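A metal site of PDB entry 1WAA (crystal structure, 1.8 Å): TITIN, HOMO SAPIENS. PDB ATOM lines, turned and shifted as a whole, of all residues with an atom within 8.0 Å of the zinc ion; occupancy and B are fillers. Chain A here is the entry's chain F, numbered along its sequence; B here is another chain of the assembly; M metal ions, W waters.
Water W1 lies within hydrogen-bond range of OH of Tyr 13 of chain B (3.2 Å), NZ of Lys 59 of chain B (3.3 Å) and OE2 of Glu 52 (3.3 Å).
The side-chain carboxylate (OE2) of Glu 52 lies within salt-bridge range of the side-chain amino group (NZ) of Lys 59 of chain B, at 2.5 Å.
O of Glu 52 sits at hydrogen-bond distance from N of Ile 63, at 2.9 Å.
N of His 65 sits at hydrogen-bond distance from O of Asp 50, 2.8 Å away.
The side-chain carboxylate (OE2) of Glu 26 of chain B lies close to the side-chain amino group (NZ) of Lys 59 of chain B, 3.2 Å away.
OE2 of Glu 28 of chain B lies within salt-bridge range of NZ of Lys 59 of chain B.
Lys 59 of chain B touches the zinc ion (NZ to ZN, 3.6 Å).
Four residues have an atom within 4 Å of the zinc ion: Glu 52, His 65, Glu 26 of chain B and Lys 59 of chain B.
The zinc ion is bound by OE1 of Glu 52 (1.9 Å).
NE2 of His 65 binds the zinc ion (2.0 Å).
Water W1 is bound to the zinc ion, 2.1 Å away.
OE1 of Glu 26 of chain B binds the zinc ion (2.2 Å).
The zinc ion is bound by the side-chain carboxylate (OE2) of Glu 26 of chain B (2.6 Å).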
ATOM      1  N   THR A  22       1.400 -22.846 -15.659  1.00  0.00           N
ATOM      2  CA  THR A  22       1.734 -21.443 -15.409  1.00  0.00           C
ATOM      3  C   THR A  22       2.449 -21.187 -14.075  1.00  0.00           C
ATOM      4  O   THR A  22       2.154 -21.802 -13.065  1.00  0.00           O
ATOM      5  CB  THR A  22       0.540 -20.479 -15.704  1.00  0.00           C
ATOM      6  OG1 THR A  22       0.391 -19.508 -14.660  1.00  0.00           O
ATOM      7  CG2 THR A  22      -0.708 -21.190 -15.835  1.00  0.00           C
ATOM      8  N   HIS A  24       3.693 -18.125 -11.369  1.00  0.00           N
ATOM      9  CA  HIS A  24       3.292 -16.812 -10.917  1.00  0.00           C
ATOM     10  C   HIS A  24       4.350 -16.329  -9.942  1.00  0.00           C
ATOM     11  O   HIS A  24       4.670 -17.041  -8.958  1.00  0.00           O
ATOM     12  CB  HIS A  24       1.960 -16.860 -10.169  1.00  0.00           C
ATOM     13  CG  HIS A  24       0.825 -17.451 -10.945  1.00  0.00           C
ATOM     14  ND1 HIS A  24       0.514 -18.794 -10.913  1.00  0.00           N
ATOM     15  CD2 HIS A  24      -0.088 -16.874 -11.768  1.00  0.00           C
ATOM     16  CE1 HIS A  24      -0.544 -19.022 -11.666  1.00  0.00           C
ATOM     17  NE2 HIS A  24      -0.938 -17.872 -12.197  1.00  0.00           N
ATOM     18  N   SER A  48       3.519 -10.457 -24.127  1.00  0.00           N
ATOM     19  CA  SER A  48       2.521 -11.345 -24.782  1.00  0.00           C
ATOM     20  C   SER A  48       1.312 -11.896 -23.949  1.00  0.00           C
ATOM     21  O   SER A  48       1.174 -11.613 -22.752  1.00  0.00           O
ATOM     22  CB  SER A  48       3.269 -12.532 -25.368  1.00  0.00           C
ATOM     23  OG  SER A  48       3.639 -13.426 -24.332  1.00  0.00           O
ATOM     24  N   PRO A  49       0.420 -12.678 -24.596  1.00  0.00           N
ATOM     25  CA  PRO A  49      -0.621 -13.405 -23.825  1.00  0.00           C
ATOM     26  C   PRO A  49      -0.060 -14.432 -22.841  1.00  0.00           C
ATOM     27  O   PRO A  49      -0.705 -14.674 -21.804  1.00  0.00           O
ATOM     28  CB  PRO A  49      -1.459 -14.111 -24.910  1.00  0.00           C
ATOM     29  CG  PRO A  49      -1.129 -13.412 -26.171  1.00  0.00           C
ATOM     30  CD  PRO A  49       0.274 -12.908 -26.045  1.00  0.00           C
ATOM     31  N   ASP A  50       1.110 -15.001 -23.141  1.00  0.00           N
ATOM     32  CA  ASP A  50       1.769 -15.951 -22.261  1.00  0.00           C
ATOM     33  C   ASP A  50       2.681 -15.331 -21.206  1.00  0.00           C
ATOM     34  O   ASP A  50       3.237 -16.036 -20.343  1.00  0.00           O
ATOM     35  CB  ASP A  50       2.584 -16.940 -23.100  1.00  0.00           C
ATOM     36  CG  ASP A  50       1.723 -18.029 -23.749  1.00  0.00           C
ATOM     37  OD1 ASP A  50       0.511 -18.144 -23.424  1.00  0.00           O
ATOM     38  OD2 ASP A  50       2.234 -18.794 -24.594  1.00  0.00           O
ATOM     39  N   CYS A  51       2.860 -14.015 -21.274  1.00  0.00           N
ATOM     40  CA  CYS A  51       3.764 -13.308 -20.363  1.00  0.00           C
ATOM     41  C   CYS A  51       3.119 -11.997 -19.924  1.00  0.00           C
ATOM     42  O   CYS A  51       3.132 -10.997 -20.645  1.00  0.00           O
ATOM     43  CB  CYS A  51       5.115 -13.087 -21.045  1.00  0.00           C
ATOM     44  SG  CYS A  51       6.322 -12.273 -19.990  1.00  0.00           S
ATOM     45  N   GLU A  52       2.503 -12.007 -18.743  1.00  0.00           N
ATOM     46  CA  GLU A  52       1.654 -10.899 -18.291  1.00  0.00           C
ATOM     47  C   GLU A  52       2.304 -10.204 -17.105  1.00  0.00           C
ATOM     48  O   GLU A  52       2.629 -10.841 -16.119  1.00  0.00           O
ATOM     49  CB  GLU A  52       0.264 -11.417 -17.930  1.00  0.00           C
ATOM     50  CG  GLU A  52      -0.511 -11.856 -19.171  1.00  0.00           C
ATOM     51  CD  GLU A  52      -1.778 -12.634 -18.854  1.00  0.00           C
ATOM     52  OE1 GLU A  52      -1.725 -13.619 -18.096  1.00  0.00           O
ATOM     53  OE2 GLU A  52      -2.832 -12.297 -19.421  1.00  0.00           O
ATOM     54  N   ILE A  54       1.996  -7.320 -14.227  1.00  0.00           N
ATOM     55  CA  ILE A  54       0.906  -6.768 -13.451  1.00  0.00           C
ATOM     56  C   ILE A  54       1.437  -5.907 -12.299  1.00  0.00           C
ATOM     57  O   ILE A  54       2.455  -6.233 -11.658  1.00  0.00           O
ATOM     58  CB  ILE A  54       0.022  -7.948 -12.910  1.00  0.00           C
ATOM     59  CG1 ILE A  54      -0.868  -8.504 -14.049  1.00  0.00           C
ATOM     60  CG2 ILE A  54      -0.869  -7.547 -11.743  1.00  0.00           C
ATOM     61  CD1 ILE A  54      -0.737  -9.965 -14.190  1.00  0.00           C
ATOM     62  N   ILE A  63       3.126 -13.222 -14.520  1.00  0.00           N
ATOM     63  CA  ILE A  63       2.486 -14.521 -14.869  1.00  0.00           C
ATOM     64  C   ILE A  63       3.076 -15.079 -16.167  1.00  0.00           C
ATOM     65  O   ILE A  63       3.087 -14.407 -17.190  1.00  0.00           O
ATOM     66  CB  ILE A  63       0.952 -14.401 -15.044  1.00  0.00           C
ATOM     67  CG1 ILE A  63       0.327 -13.749 -13.797  1.00  0.00           C
ATOM     68  CG2 ILE A  63       0.349 -15.785 -15.320  1.00  0.00           C
ATOM     69  CD1 ILE A  63      -1.184 -13.531 -13.876  1.00  0.00           C
ATOM     70  N   LEU A  64       3.542 -16.308 -16.108  1.00  0.00           N
ATOM     71  CA  LEU A  64       4.113 -16.975 -17.274  1.00  0.00           C
ATOM     72  C   LEU A  64       3.314 -18.212 -17.575  1.00  0.00           C
ATOM     73  O   LEU A  64       3.377 -19.167 -16.820  1.00  0.00           O
ATOM     74  CB  LEU A  64       5.567 -17.366 -17.044  1.00  0.00           C
ATOM     75  CG  LEU A  64       6.488 -16.236 -16.639  1.00  0.00           C
ATOM     76  CD1 LEU A  64       7.785 -16.783 -16.051  1.00  0.00           C
ATOM     77  CD2 LEU A  64       6.788 -15.383 -17.844  1.00  0.00           C
ATOM     78  N   HIS A  65       2.546 -18.164 -18.663  1.00  0.00           N
ATOM     79  CA  HIS A  65       1.732 -19.311 -19.103  1.00  0.00           C
ATOM     80  C   HIS A  65       2.540 -20.232 -19.993  1.00  0.00           C
ATOM     81  O   HIS A  65       3.477 -19.801 -20.673  1.00  0.00           O
ATOM     82  CB  HIS A  65       0.498 -18.867 -19.886  1.00  0.00           C
ATOM     83  CG  HIS A  65      -0.483 -18.090 -19.071  1.00  0.00           C
ATOM     84  ND1 HIS A  65      -1.130 -18.624 -17.980  1.00  0.00           N
ATOM     85  CD2 HIS A  65      -0.923 -16.816 -19.174  1.00  0.00           C
ATOM     86  CE1 HIS A  65      -1.929 -17.719 -17.446  1.00  0.00           C
ATOM     87  NE2 HIS A  65      -1.832 -16.609 -18.157  1.00  0.00           N
ATOM     88  N   LYS B  10     -11.730 -14.275 -19.949  1.00  0.00           N
ATOM     89  CA  LYS B  10     -10.841 -15.390 -19.595  1.00  0.00           C
ATOM     90  C   LYS B  10     -11.280 -15.900 -18.244  1.00  0.00           C
ATOM     91  O   LYS B  10     -11.061 -15.224 -17.246  1.00  0.00           O
ATOM     92  CB  LYS B  10      -9.379 -14.912 -19.518  1.00  0.00           C
ATOM     93  CG  LYS B  10      -8.586 -15.132 -20.814  1.00  0.00           C
ATOM     94  CD  LYS B  10      -7.752 -13.924 -21.212  1.00  0.00           C
ATOM     95  CE  LYS B  10      -7.552 -13.864 -22.736  1.00  0.00           C
ATOM     96  N   TYR B  13      -9.274 -20.559 -14.037  1.00  0.00           N
ATOM     97  CA  TYR B  13      -8.842 -21.940 -14.140  1.00  0.00           C
ATOM     98  C   TYR B  13      -8.664 -22.523 -12.747  1.00  0.00           C
ATOM     99  O   TYR B  13      -8.303 -21.811 -11.799  1.00  0.00           O
ATOM    100  CB  TYR B  13      -7.499 -22.101 -14.865  1.00  0.00           C
ATOM    101  CG  TYR B  13      -7.057 -21.025 -15.854  1.00  0.00           C
ATOM    102  CD1 TYR B  13      -7.148 -21.240 -17.245  1.00  0.00           C
ATOM    103  CD2 TYR B  13      -6.426 -19.844 -15.391  1.00  0.00           C
ATOM    104  CE1 TYR B  13      -6.683 -20.274 -18.171  1.00  0.00           C
ATOM    105  CE2 TYR B  13      -5.962 -18.849 -16.298  1.00  0.00           C
ATOM    106  CZ  TYR B  13      -6.086 -19.066 -17.678  1.00  0.00           C
ATOM    107  OH  TYR B  13      -5.634 -18.096 -18.570  1.00  0.00           O
ATOM    108  N   GLU B  26      -6.694 -16.189 -11.501  1.00  0.00           N
ATOM    109  CA  GLU B  26      -6.828 -14.981 -12.325  1.00  0.00           C
ATOM    110  C   GLU B  26      -7.993 -15.136 -13.272  1.00  0.00           C
ATOM    111  O   GLU B  26      -8.287 -16.235 -13.760  1.00  0.00           O
ATOM    112  CB  GLU B  26      -5.549 -14.590 -13.127  1.00  0.00           C
ATOM    113  CG  GLU B  26      -5.012 -15.667 -14.019  1.00  0.00           C
ATOM    114  CD  GLU B  26      -4.288 -15.189 -15.290  1.00  0.00           C
ATOM    115  OE1 GLU B  26      -3.635 -16.051 -15.907  1.00  0.00           O
ATOM    116  OE2 GLU B  26      -4.336 -13.990 -15.731  1.00  0.00           O
ATOM    117  N   ILE B  27      -8.644 -14.014 -13.485  1.00  0.00           N
ATOM    118  CA  ILE B  27      -9.772 -13.911 -14.390  1.00  0.00           C
ATOM    119  C   ILE B  27      -9.650 -12.574 -15.117  1.00  0.00           C
ATOM    120  O   ILE B  27      -9.182 -11.568 -14.553  1.00  0.00           O
ATOM    121  CB  ILE B  27     -11.114 -14.021 -13.580  1.00  0.00           C
ATOM    122  CG1 ILE B  27     -12.337 -13.869 -14.506  1.00  0.00           C
ATOM    123  CG2 ILE B  27     -11.197 -12.998 -12.459  1.00  0.00           C
ATOM    124  CD1 ILE B  27     -13.648 -13.993 -13.779  1.00  0.00           C
ATOM    125  N   GLU B  28     -10.043 -12.572 -16.388  1.00  0.00           N
ATOM    126  CA  GLU B  28     -10.016 -11.353 -17.179  1.00  0.00           C
ATOM    127  C   GLU B  28     -11.442 -10.989 -17.586  1.00  0.00           C
ATOM    128  O   GLU B  28     -12.199 -11.824 -18.063  1.00  0.00           O
ATOM    129  CB  GLU B  28      -9.171 -11.509 -18.429  1.00  0.00           C
ATOM    130  CG  GLU B  28      -9.064 -10.207 -19.199  1.00  0.00           C
ATOM    131  CD  GLU B  28      -8.081 -10.284 -20.355  1.00  0.00           C
ATOM    132  OE1 GLU B  28      -8.511 -10.064 -21.518  1.00  0.00           O
ATOM    133  OE2 GLU B  28      -6.863 -10.582 -20.144  1.00  0.00           O
ATOM    134  N   LYS B  59      -7.789  -7.343 -15.452  1.00  0.00           N
ATOM    135  CA  LYS B  59      -7.394  -8.513 -14.687  1.00  0.00           C
ATOM    136  C   LYS B  59      -7.782  -8.441 -13.227  1.00  0.00           C
ATOM    137  O   LYS B  59      -7.666  -7.393 -12.597  1.00  0.00           O
ATOM    138  CB  LYS B  59      -5.863  -8.670 -14.753  1.00  0.00           C
ATOM    139  CG  LYS B  59      -5.373  -9.064 -16.112  1.00  0.00           C
ATOM    140  CD  LYS B  59      -5.667 -10.529 -16.400  1.00  0.00           C
ATOM    141  CE  LYS B  59      -4.516 -11.177 -17.119  1.00  0.00           C
ATOM    142  NZ  LYS B  59      -5.001 -12.055 -18.186  1.00  0.00           N
ATOM    143  N   ILE B  61      -6.986 -10.792  -9.732  1.00  0.00           N
ATOM    144  CA  ILE B  61      -6.176 -11.893  -9.198  1.00  0.00           C
ATOM    145  C   ILE B  61      -6.381 -12.051  -7.681  1.00  0.00           C
ATOM    146  O   ILE B  61      -6.558 -11.064  -6.950  1.00  0.00           O
ATOM    147  CB  ILE B  61      -4.681 -11.622  -9.518  1.00  0.00           C
ATOM    148  CG1 ILE B  61      -4.429 -11.762 -11.038  1.00  0.00           C
ATOM    149  CG2 ILE B  61      -3.710 -12.544  -8.732  1.00  0.00           C
ATOM    150  CD1 ILE B  61      -3.233 -10.976 -11.534  1.00  0.00           C
HETATM  151 ZN    ZN M   1      -3.015 -15.018 -17.720  1.00  0.00          ZN
HETATM  152  O   HOH W   1      -4.523 -15.171 -19.140  1.00  0.00           O
